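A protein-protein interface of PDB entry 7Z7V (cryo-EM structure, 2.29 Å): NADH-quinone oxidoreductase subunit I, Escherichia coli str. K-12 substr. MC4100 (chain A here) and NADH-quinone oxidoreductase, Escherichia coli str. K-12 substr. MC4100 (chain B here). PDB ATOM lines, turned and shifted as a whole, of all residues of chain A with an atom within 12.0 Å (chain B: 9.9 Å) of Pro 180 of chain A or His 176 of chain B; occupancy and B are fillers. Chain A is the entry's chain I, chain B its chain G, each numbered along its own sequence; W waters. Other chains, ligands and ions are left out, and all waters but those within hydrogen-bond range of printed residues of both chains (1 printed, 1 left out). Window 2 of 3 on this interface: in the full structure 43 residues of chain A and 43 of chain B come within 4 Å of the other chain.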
ATOM      1  N   ALA A 170      27.229 -12.043 -25.732  1.00  0.00           N
ATOM      2  CA  ALA A 170      27.976 -11.285 -24.750  1.00  0.00           C
ATOM      3  C   ALA A 170      28.011 -12.042 -23.429  1.00  0.00           C
ATOM      4  O   ALA A 170      27.194 -12.929 -23.172  1.00  0.00           O
ATOM      5  CB  ALA A 170      27.363  -9.901 -24.552  1.00  0.00           C
ATOM      6  N   LYS A 171      28.984 -11.695 -22.596  1.00  0.00           N
ATOM      7  CA  LYS A 171      29.067 -12.279 -21.269  1.00  0.00           C
ATOM      8  C   LYS A 171      27.883 -11.814 -20.421  1.00  0.00           C
ATOM      9  O   LYS A 171      27.383 -10.702 -20.602  1.00  0.00           O
ATOM     10  CB  LYS A 171      30.377 -11.888 -20.592  1.00  0.00           C
ATOM     11  CG  LYS A 171      31.315 -13.051 -20.354  1.00  0.00           C
ATOM     12  CD  LYS A 171      31.745 -13.691 -21.661  1.00  0.00           C
ATOM     13  CE  LYS A 171      32.482 -14.999 -21.418  1.00  0.00           C
ATOM     14  NZ  LYS A 171      31.607 -16.011 -20.761  1.00  0.00           N
ATOM     15  N   PRO A 172      27.395 -12.662 -19.516  1.00  0.00           N
ATOM     16  CA  PRO A 172      26.264 -12.260 -18.671  1.00  0.00           C
ATOM     17  C   PRO A 172      26.655 -11.150 -17.709  1.00  0.00           C
ATOM     18  O   PRO A 172      27.712 -11.196 -17.078  1.00  0.00           O
ATOM     19  CB  PRO A 172      25.892 -13.550 -17.930  1.00  0.00           C
ATOM     20  CG  PRO A 172      27.084 -14.419 -18.040  1.00  0.00           C
ATOM     21  CD  PRO A 172      27.748 -14.078 -19.327  1.00  0.00           C
ATOM     22  N   ILE A 173      25.797 -10.142 -17.616  1.00  0.00           N
ATOM     23  CA  ILE A 173      25.992  -9.007 -16.723  1.00  0.00           C
ATOM     24  C   ILE A 173      25.022  -9.167 -15.567  1.00  0.00           C
ATOM     25  O   ILE A 173      23.802  -9.194 -15.770  1.00  0.00           O
ATOM     26  CB  ILE A 173      25.772  -7.669 -17.443  1.00  0.00           C
ATOM     27  CG1 ILE A 173      26.788  -7.491 -18.569  1.00  0.00           C
ATOM     28  CG2 ILE A 173      25.851  -6.513 -16.459  1.00  0.00           C
ATOM     29  CD1 ILE A 173      26.323  -6.564 -19.660  1.00  0.00           C
ATOM     30  N   ASP A 174      25.561  -9.285 -14.359  1.00  0.00           N
ATOM     31  CA  ASP A 174      24.730  -9.409 -13.175  1.00  0.00           C
ATOM     32  C   ASP A 174      23.975  -8.110 -12.922  1.00  0.00           C
ATOM     33  O   ASP A 174      24.474  -7.015 -13.189  1.00  0.00           O
ATOM     34  CB  ASP A 174      25.587  -9.768 -11.960  1.00  0.00           C
ATOM     35  CG  ASP A 174      24.795 -10.459 -10.871  1.00  0.00           C
ATOM     36  OD1 ASP A 174      25.059 -11.648 -10.605  1.00  0.00           O
ATOM     37  OD2 ASP A 174      23.909  -9.815 -10.276  1.00  0.00           O
ATOM     38  N   VAL A 175      22.751  -8.241 -12.406  1.00  0.00           N
ATOM     39  CA  VAL A 175      21.960  -7.064 -12.069  1.00  0.00           C
ATOM     40  C   VAL A 175      22.546  -6.316 -10.882  1.00  0.00           C
ATOM     41  O   VAL A 175      22.215  -5.146 -10.668  1.00  0.00           O
ATOM     42  CB  VAL A 175      20.496  -7.446 -11.787  1.00  0.00           C
ATOM     43  CG1 VAL A 175      19.806  -7.860 -13.068  1.00  0.00           C
ATOM     44  CG2 VAL A 175      20.423  -8.546 -10.746  1.00  0.00           C
ATOM     45  N   LYS A 176      23.418  -6.958 -10.113  1.00  0.00           N
ATOM     46  CA  LYS A 176      24.097  -6.339  -8.987  1.00  0.00           C
ATOM     47  C   LYS A 176      25.381  -5.626  -9.388  1.00  0.00           C
ATOM     48  O   LYS A 176      26.105  -5.150  -8.510  1.00  0.00           O
ATOM     49  CB  LYS A 176      24.407  -7.397  -7.925  1.00  0.00           C
ATOM     50  CG  LYS A 176      23.185  -7.895  -7.182  1.00  0.00           C
ATOM     51  CD  LYS A 176      23.277  -9.374  -6.890  1.00  0.00           C
ATOM     52  CE  LYS A 176      24.281  -9.651  -5.793  1.00  0.00           C
ATOM     53  NZ  LYS A 176      25.135 -10.828  -6.110  1.00  0.00           N
ATOM     54  N   SER A 177      25.683  -5.546 -10.682  1.00  0.00           N
ATOM     55  CA  SER A 177      26.919  -4.922 -11.133  1.00  0.00           C
ATOM     56  C   SER A 177      26.876  -3.411 -10.932  1.00  0.00           C
ATOM     57  O   SER A 177      25.824  -2.776 -11.030  1.00  0.00           O
ATOM     58  CB  SER A 177      27.178  -5.244 -12.604  1.00  0.00           C
ATOM     59  OG  SER A 177      26.545  -4.310 -13.455  1.00  0.00           O
ATOM     60  N   LEU A 178      28.047  -2.839 -10.650  1.00  0.00           N
ATOM     61  CA  LEU A 178      28.139  -1.419 -10.332  1.00  0.00           C
ATOM     62  C   LEU A 178      28.031  -0.528 -11.560  1.00  0.00           C
ATOM     63  O   LEU A 178      27.742   0.663 -11.416  1.00  0.00           O
ATOM     64  CB  LEU A 178      29.453  -1.129  -9.609  1.00  0.00           C
ATOM     65  CG  LEU A 178      29.814  -2.051  -8.446  1.00  0.00           C
ATOM     66  CD1 LEU A 178      31.274  -1.890  -8.078  1.00  0.00           C
ATOM     67  CD2 LEU A 178      28.923  -1.764  -7.255  1.00  0.00           C
ATOM     68  N   LEU A 179      28.262  -1.064 -12.747  1.00  0.00           N
ATOM     69  CA  LEU A 179      28.224  -0.249 -13.953  1.00  0.00           C
ATOM     70  C   LEU A 179      26.784   0.121 -14.287  1.00  0.00           C
ATOM     71  O   LEU A 179      25.903  -0.743 -14.238  1.00  0.00           O
ATOM     72  CB  LEU A 179      28.869  -0.994 -15.117  1.00  0.00           C
ATOM     73  CG  LEU A 179      30.397  -1.026 -15.093  1.00  0.00           C
ATOM     74  CD1 LEU A 179      30.932  -1.888 -16.218  1.00  0.00           C
ATOM     75  CD2 LEU A 179      30.954   0.381 -15.183  1.00  0.00           C
ATOM     76  N   PRO A 180      26.501   1.390 -14.627  1.00  0.00           N
ATOM     77  CA  PRO A 180      25.145   1.875 -14.912  1.00  0.00           C
ATOM     78  C   PRO A 180      24.518   1.226 -16.146  1.00  0.00           C
ATOM     79  O   PRO A 180      25.235   0.886 -17.085  1.00  0.00           O
ATOM     80  CB  PRO A 180      25.346   3.378 -15.142  1.00  0.00           C
ATOM     81  CG  PRO A 180      26.709   3.688 -14.624  1.00  0.00           C
ATOM     82  CD  PRO A 180      27.505   2.450 -14.801  1.00  0.00           C
ATOM     83  N   ASN B  98      18.234 -10.183 -29.074  1.00  0.00           N
ATOM     84  CA  ASN B  98      18.902 -10.857 -27.972  1.00  0.00           C
ATOM     85  C   ASN B  98      18.407 -12.275 -27.735  1.00  0.00           C
ATOM     86  O   ASN B  98      18.883 -12.928 -26.804  1.00  0.00           O
ATOM     87  CB  ASN B  98      18.732 -10.047 -26.689  1.00  0.00           C
ATOM     88  CG  ASN B  98      19.399  -8.700 -26.764  1.00  0.00           C
ATOM     89  OD1 ASN B  98      20.600  -8.603 -27.002  1.00  0.00           O
ATOM     90  ND2 ASN B  98      18.624  -7.648 -26.560  1.00  0.00           N
ATOM     91  N   ARG B 133      22.637 -10.327 -25.463  1.00  0.00           N
ATOM     92  CA  ARG B 133      22.785 -10.348 -24.018  1.00  0.00           C
ATOM     93  C   ARG B 133      22.456 -11.735 -23.475  1.00  0.00           C
ATOM     94  O   ARG B 133      21.671 -12.487 -24.055  1.00  0.00           O
ATOM     95  CB  ARG B 133      21.897  -9.290 -23.358  1.00  0.00           C
ATOM     96  CG  ARG B 133      20.405  -9.527 -23.481  1.00  0.00           C
ATOM     97  CD  ARG B 133      19.804 -10.021 -22.176  1.00  0.00           C
ATOM     98  NE  ARG B 133      18.404 -10.405 -22.309  1.00  0.00           N
ATOM     99  CZ  ARG B 133      17.977 -11.559 -22.806  1.00  0.00           C
ATOM    100  NH1 ARG B 133      18.818 -12.470 -23.265  1.00  0.00           N
ATOM    101  NH2 ARG B 133      16.673 -11.802 -22.847  1.00  0.00           N
ATOM    102  N   HIS B 135      21.974 -14.209 -19.722  1.00  0.00           N
ATOM    103  CA  HIS B 135      21.684 -14.239 -18.298  1.00  0.00           C
ATOM    104  C   HIS B 135      22.003 -15.610 -17.721  1.00  0.00           C
ATOM    105  O   HIS B 135      21.891 -16.630 -18.403  1.00  0.00           O
ATOM    106  CB  HIS B 135      20.218 -13.918 -18.020  1.00  0.00           C
ATOM    107  CG  HIS B 135      19.845 -12.494 -18.280  1.00  0.00           C
ATOM    108  ND1 HIS B 135      20.315 -11.451 -17.517  1.00  0.00           N
ATOM    109  CD2 HIS B 135      19.027 -11.944 -19.206  1.00  0.00           C
ATOM    110  CE1 HIS B 135      19.811 -10.317 -17.966  1.00  0.00           C
ATOM    111  NE2 HIS B 135      19.023 -10.589 -18.989  1.00  0.00           N
ATOM    112  N   MET B 148      16.479 -17.530 -18.338  1.00  0.00           N
ATOM    113  CA  MET B 148      16.261 -16.101 -18.521  1.00  0.00           C
ATOM    114  C   MET B 148      16.777 -15.564 -19.848  1.00  0.00           C
ATOM    115  O   MET B 148      16.467 -14.418 -20.182  1.00  0.00           O
ATOM    116  CB  MET B 148      16.900 -15.318 -17.372  1.00  0.00           C
ATOM    117  CG  MET B 148      15.902 -14.828 -16.339  1.00  0.00           C
ATOM    118  SD  MET B 148      14.720 -13.591 -16.914  1.00  0.00           S
ATOM    119  CE  MET B 148      15.788 -12.415 -17.733  1.00  0.00           C
ATOM    120  N   CYS B 151      13.888 -14.520 -22.217  1.00  0.00           N
ATOM    121  CA  CYS B 151      12.931 -13.523 -21.761  1.00  0.00           C
ATOM    122  C   CYS B 151      12.822 -12.368 -22.742  1.00  0.00           C
ATOM    123  O   CYS B 151      13.821 -11.895 -23.284  1.00  0.00           O
ATOM    124  CB  CYS B 151      13.333 -13.012 -20.384  1.00  0.00           C
ATOM    125  SG  CYS B 151      12.278 -11.738 -19.736  1.00  0.00           S
ATOM    126  N   ILE B 152      11.593 -11.920 -22.971  1.00  0.00           N
ATOM    127  CA  ILE B 152      11.325 -10.768 -23.817  1.00  0.00           C
ATOM    128  C   ILE B 152      10.888  -9.562 -23.001  1.00  0.00           C
ATOM    129  O   ILE B 152      10.470  -8.556 -23.579  1.00  0.00           O
ATOM    130  CB  ILE B 152      10.288 -11.096 -24.902  1.00  0.00           C
ATOM    131  CG1 ILE B 152       8.965 -11.523 -24.263  1.00  0.00           C
ATOM    132  CG2 ILE B 152      10.827 -12.152 -25.850  1.00  0.00           C
ATOM    133  CD1 ILE B 152       7.893 -11.853 -25.244  1.00  0.00           C
ATOM    134  N   ALA B 153      10.983  -9.645 -21.670  1.00  0.00           N
ATOM    135  CA  ALA B 153      10.661  -8.557 -20.740  1.00  0.00           C
ATOM    136  C   ALA B 153       9.245  -8.032 -20.962  1.00  0.00           C
ATOM    137  O   ALA B 153       9.011  -6.837 -21.127  1.00  0.00           O
ATOM    138  CB  ALA B 153      11.690  -7.430 -20.827  1.00  0.00           C
ATOM    139  N   TYR B 155       6.805  -8.684 -18.732  1.00  0.00           N
ATOM    140  CA  TYR B 155       6.336  -8.450 -17.366  1.00  0.00           C
ATOM    141  C   TYR B 155       5.087  -9.243 -17.001  1.00  0.00           C
ATOM    142  O   TYR B 155       4.481  -8.960 -15.973  1.00  0.00           O
ATOM    143  CB  TYR B 155       6.091  -6.959 -17.089  1.00  0.00           C
ATOM    144  CG  TYR B 155       7.343  -6.115 -17.159  1.00  0.00           C
ATOM    145  CD1 TYR B 155       7.822  -5.651 -18.376  1.00  0.00           C
ATOM    146  CD2 TYR B 155       8.045  -5.783 -16.011  1.00  0.00           C
ATOM    147  CE1 TYR B 155       8.966  -4.893 -18.448  1.00  0.00           C
ATOM    148  CE2 TYR B 155       9.189  -5.020 -16.073  1.00  0.00           C
ATOM    149  CZ  TYR B 155       9.645  -4.579 -17.295  1.00  0.00           C
ATOM    150  OH  TYR B 155      10.783  -3.819 -17.367  1.00  0.00           O
ATOM    151  N   VAL B 172      11.207  -8.382 -10.509  1.00  0.00           N
ATOM    152  CA  VAL B 172      12.018  -7.900 -11.617  1.00  0.00           C
ATOM    153  C   VAL B 172      13.155  -7.063 -11.043  1.00  0.00           C
ATOM    154  O   VAL B 172      12.954  -6.261 -10.126  1.00  0.00           O
ATOM    155  CB  VAL B 172      11.166  -7.107 -12.637  1.00  0.00           C
ATOM    156  CG1 VAL B 172      10.326  -6.037 -11.956  1.00  0.00           C
ATOM    157  CG2 VAL B 172      12.025  -6.513 -13.745  1.00  0.00           C
ATOM    158  N   TYR B 173      14.358  -7.289 -11.557  1.00  0.00           N
ATOM    159  CA  TYR B 173      15.580  -6.678 -11.063  1.00  0.00           C
ATOM    160  C   TYR B 173      16.346  -6.060 -12.222  1.00  0.00           C
ATOM    161  O   TYR B 173      16.089  -6.357 -13.388  1.00  0.00           O
ATOM    162  CB  TYR B 173      16.440  -7.709 -10.324  1.00  0.00           C
ATOM    163  CG  TYR B 173      15.605  -8.629  -9.479  1.00  0.00           C
ATOM    164  CD1 TYR B 173      15.050  -8.185  -8.290  1.00  0.00           C
ATOM    165  CD2 TYR B 173      15.328  -9.921  -9.891  1.00  0.00           C
ATOM    166  CE1 TYR B 173      14.267  -9.007  -7.522  1.00  0.00           C
ATOM    167  CE2 TYR B 173      14.545 -10.751  -9.130  1.00  0.00           C
ATOM    168  CZ  TYR B 173      14.017 -10.289  -7.946  1.00  0.00           C
ATOM    169  OH  TYR B 173      13.234 -11.111  -7.185  1.00  0.00           O
ATOM    170  N   GLY B 174      17.278  -5.182 -11.892  1.00  0.00           N
ATOM    171  CA  GLY B 174      18.060  -4.515 -12.904  1.00  0.00           C
ATOM    172  C   GLY B 174      17.294  -3.409 -13.602  1.00  0.00           C
ATOM    173  O   GLY B 174      16.243  -2.949 -13.157  1.00  0.00           O
ATOM    174  N   ALA B 175      17.854  -2.975 -14.727  1.00  0.00           N
ATOM    175  CA  ALA B 175      17.279  -1.894 -15.513  1.00  0.00           C
ATOM    176  C   ALA B 175      17.724  -2.059 -16.959  1.00  0.00           C
ATOM    177  O   ALA B 175      18.488  -2.970 -17.286  1.00  0.00           O
ATOM    178  CB  ALA B 175      17.681  -0.527 -14.952  1.00  0.00           C
ATOM    179  N   HIS B 176      17.282  -1.117 -17.805  1.00  0.00           N
ATOM    180  CA  HIS B 176      17.409  -1.097 -19.267  1.00  0.00           C
ATOM    181  C   HIS B 176      17.259  -2.480 -19.893  1.00  0.00           C
ATOM    182  O   HIS B 176      16.294  -3.190 -19.598  1.00  0.00           O
ATOM    183  CB  HIS B 176      18.725  -0.428 -19.710  1.00  0.00           C
ATOM    184  CG  HIS B 176      19.926  -0.807 -18.903  1.00  0.00           C
ATOM    185  ND1 HIS B 176      20.766  -1.839 -19.259  1.00  0.00           N
ATOM    186  CD2 HIS B 176      20.427  -0.293 -17.756  1.00  0.00           C
ATOM    187  CE1 HIS B 176      21.732  -1.945 -18.365  1.00  0.00           C
ATOM    188  NE2 HIS B 176      21.549  -1.019 -17.442  1.00  0.00           N
ATOM    189  N   ASP B 177      18.199  -2.886 -20.739  1.00  0.00           N
ATOM    190  CA  ASP B 177      18.091  -4.184 -21.392  1.00  0.00           C
ATOM    191  C   ASP B 177      18.603  -5.325 -20.525  1.00  0.00           C
ATOM    192  O   ASP B 177      18.663  -6.462 -20.995  1.00  0.00           O
ATOM    193  CB  ASP B 177      18.824  -4.177 -22.738  1.00  0.00           C
ATOM    194  CG  ASP B 177      20.286  -3.800 -22.615  1.00  0.00           C
ATOM    195  OD1 ASP B 177      20.715  -3.355 -21.534  1.00  0.00           O
ATOM    196  OD2 ASP B 177      21.012  -3.948 -23.617  1.00  0.00           O
ATOM    197  N   ASN B 178      18.974  -5.052 -19.277  1.00  0.00           N
ATOM    198  CA  ASN B 178      19.436  -6.076 -18.355  1.00  0.00           C
ATOM    199  C   ASN B 178      18.395  -6.406 -17.289  1.00  0.00           C
ATOM    200  O   ASN B 178      18.749  -6.818 -16.184  1.00  0.00           O
ATOM    201  CB  ASN B 178      20.747  -5.647 -17.703  1.00  0.00           C
ATOM    202  CG  ASN B 178      21.617  -6.821 -17.328  1.00  0.00           C
ATOM    203  OD1 ASN B 178      21.702  -7.799 -18.062  1.00  0.00           O
ATOM    204  ND2 ASN B 178      22.262  -6.734 -16.175  1.00  0.00           N
ATOM    205  N   VAL B 179      17.111  -6.227 -17.598  1.00  0.00           N
ATOM    206  CA  VAL B 179      16.071  -6.564 -16.634  1.00  0.00           C
ATOM    207  C   VAL B 179      15.984  -8.078 -16.488  1.00  0.00           C
ATOM    208  O   VAL B 179      16.050  -8.827 -17.469  1.00  0.00           O
ATOM    209  CB  VAL B 179      14.715  -5.959 -17.033  1.00  0.00           C
ATOM    210  CG1 VAL B 179      14.642  -4.506 -16.605  1.00  0.00           C
ATOM    211  CG2 VAL B 179      14.471  -6.099 -18.520  1.00  0.00           C
ATOM    212  N   TYR B 180      15.854  -8.527 -15.249  1.00  0.00           N
ATOM    213  CA  TYR B 180      15.894  -9.929 -14.872  1.00  0.00           C
ATOM    214  C   TYR B 180      14.611 -10.274 -14.135  1.00  0.00           C
ATOM    215  O   TYR B 180      14.136  -9.495 -13.314  1.00  0.00           O
ATOM    216  CB  TYR B 180      17.107 -10.192 -13.982  1.00  0.00           C
ATOM    217  CG  TYR B 180      17.491 -11.636 -13.805  1.00  0.00           C
ATOM    218  CD1 TYR B 180      16.892 -12.418 -12.827  1.00  0.00           C
ATOM    219  CD2 TYR B 180      18.476 -12.210 -14.591  1.00  0.00           C
ATOM    220  CE1 TYR B 180      17.249 -13.734 -12.653  1.00  0.00           C
ATOM    221  CE2 TYR B 180      18.842 -13.525 -14.422  1.00  0.00           C
ATOM    222  CZ  TYR B 180      18.226 -14.281 -13.452  1.00  0.00           C
ATOM    223  OH  TYR B 180      18.586 -15.593 -13.282  1.00  0.00           O
ATOM    224  N   PHE B 181      14.047 -11.440 -14.418  1.00  0.00           N
ATOM    225  CA  PHE B 181      12.801 -11.857 -13.787  1.00  0.00           C
ATOM    226  C   PHE B 181      13.049 -13.157 -13.044  1.00  0.00           C
ATOM    227  O   PHE B 181      13.429 -14.161 -13.656  1.00  0.00           O
ATOM    228  CB  PHE B 181      11.687 -12.010 -14.823  1.00  0.00           C
ATOM    229  CG  PHE B 181      11.276 -10.714 -15.459  1.00  0.00           C
ATOM    230  CD1 PHE B 181      11.965 -10.212 -16.548  1.00  0.00           C
ATOM    231  CD2 PHE B 181      10.207  -9.992 -14.960  1.00  0.00           C
ATOM    232  CE1 PHE B 181      11.595  -9.023 -17.129  1.00  0.00           C
ATOM    233  CE2 PHE B 181       9.829  -8.804 -15.542  1.00  0.00           C
ATOM    234  CZ  PHE B 181      10.524  -8.316 -16.622  1.00  0.00           C
HETATM  235  O   HOH W   1      23.203  -9.482 -19.064  1.00  0.00           O
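Water W1 bridges the side-chain amide oxygen of Asn 178 of chain B (2.5 Å) and the backbone NH of Ile 173 of chain A (3.0 Å).
Among the printed residues, pairs that only touch across the chains: Asp 174 of chain A with Asn 178 of chain B (3.7 Å), Val 175 of chain A with Tyr 173 of chain B (3.99 Å), Val 175 of chain A with Gly 174 of chain B (3.8 Å), Val 175 of chain A with Asn 178 of chain B (3.5 Å), Val 175 of chain A with Tyr 180 of chain B (3.7 Å) and Pro 180 of chain A with His 176 of chain B (3.9 Å).
Printed residues of chain B that touch a printed residue of chain A: Tyr 173, Gly 174, His 176, Asn 178 and Tyr 180.
Hydrophobic or aromatic side chains of chain B within 4 Å of the printed part of chain A: His 176 and Tyr 180.
Of the 11 printed residues of chain A, 4 touch a printed residue of chain B.
Hydrophobic or aromatic side chains of chain A that line the printed part of chain B: Ile 173 and Val 175.
Among the printed residues, no Asp or Glu carboxylate lies within 4 Å of a Lys or Arg side-chain nitrogen of the other chain.
The backbone carbonyl oxygen of Ile 173 of chain A lies within hydrogen-bond range of the side-chain amide nitrogen of Asn 178 of chain B (2.9 Å).
Printed residues of chain B within 4 Å of Ile 173 of chain A: Asn 178.
Of the printed residues of chain B, Asp 174 of chain A touches Asn 178.
Printed residues of chain B within 4 Å of Val 175 of chain A: Tyr 173 (3.99 Å), Gly 174 (3.8 Å), Asn 178 (3.5 Å) and Tyr 180 (3.7 Å).
No residue of chain B comes within 4 Å of Leu 179 of chain A.
Of chain B, only His 176 (3.9 Å) comes within 4 Å of Pro 180 of chain A.
Of the printed residues of chain A, Tyr 173 of chain B touches Val 175 (3.99 Å).
Gly 174 of chain B touches just one residue of chain A: Val 175 (3.8 Å).
Ala 175 of chain B touches none of the printed residues of chain A.
His 176 of chain B touches one residue of chain A.
Asp 177 of chain B touches none of the printed residues of chain A.
No residue of chain A comes within 4 Å of Val 179 of chain B.
Of the printed residues of chain A, Tyr 180 of chain B touches Val 175 (3.7 Å).
The nearest residue of chain A that does not touch His 176 of chain B is Leu 179 of chain A (5.4 Å).
The backbone NH of Tyr 173 of chain B is in hydrogen-bond range of the backbone carbonyl oxygen of Tyr 180 of chain B.
A ring nitrogen (ND1) of His 176 of chain B is in hydrogen-bond range of the side-chain carboxylate of Asp 177 of chain B (2.7 Å).
OD2 of Asp 174 of chain A is in hydrogen-bond range of N of Lys 176 of chain A (2.9 Å).
The backbone carbonyl oxygen (O) of Asp 174 of chain A sits close to the side-chain hydroxyl (OG) of Ser 177 of chain A (3.4 Å).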
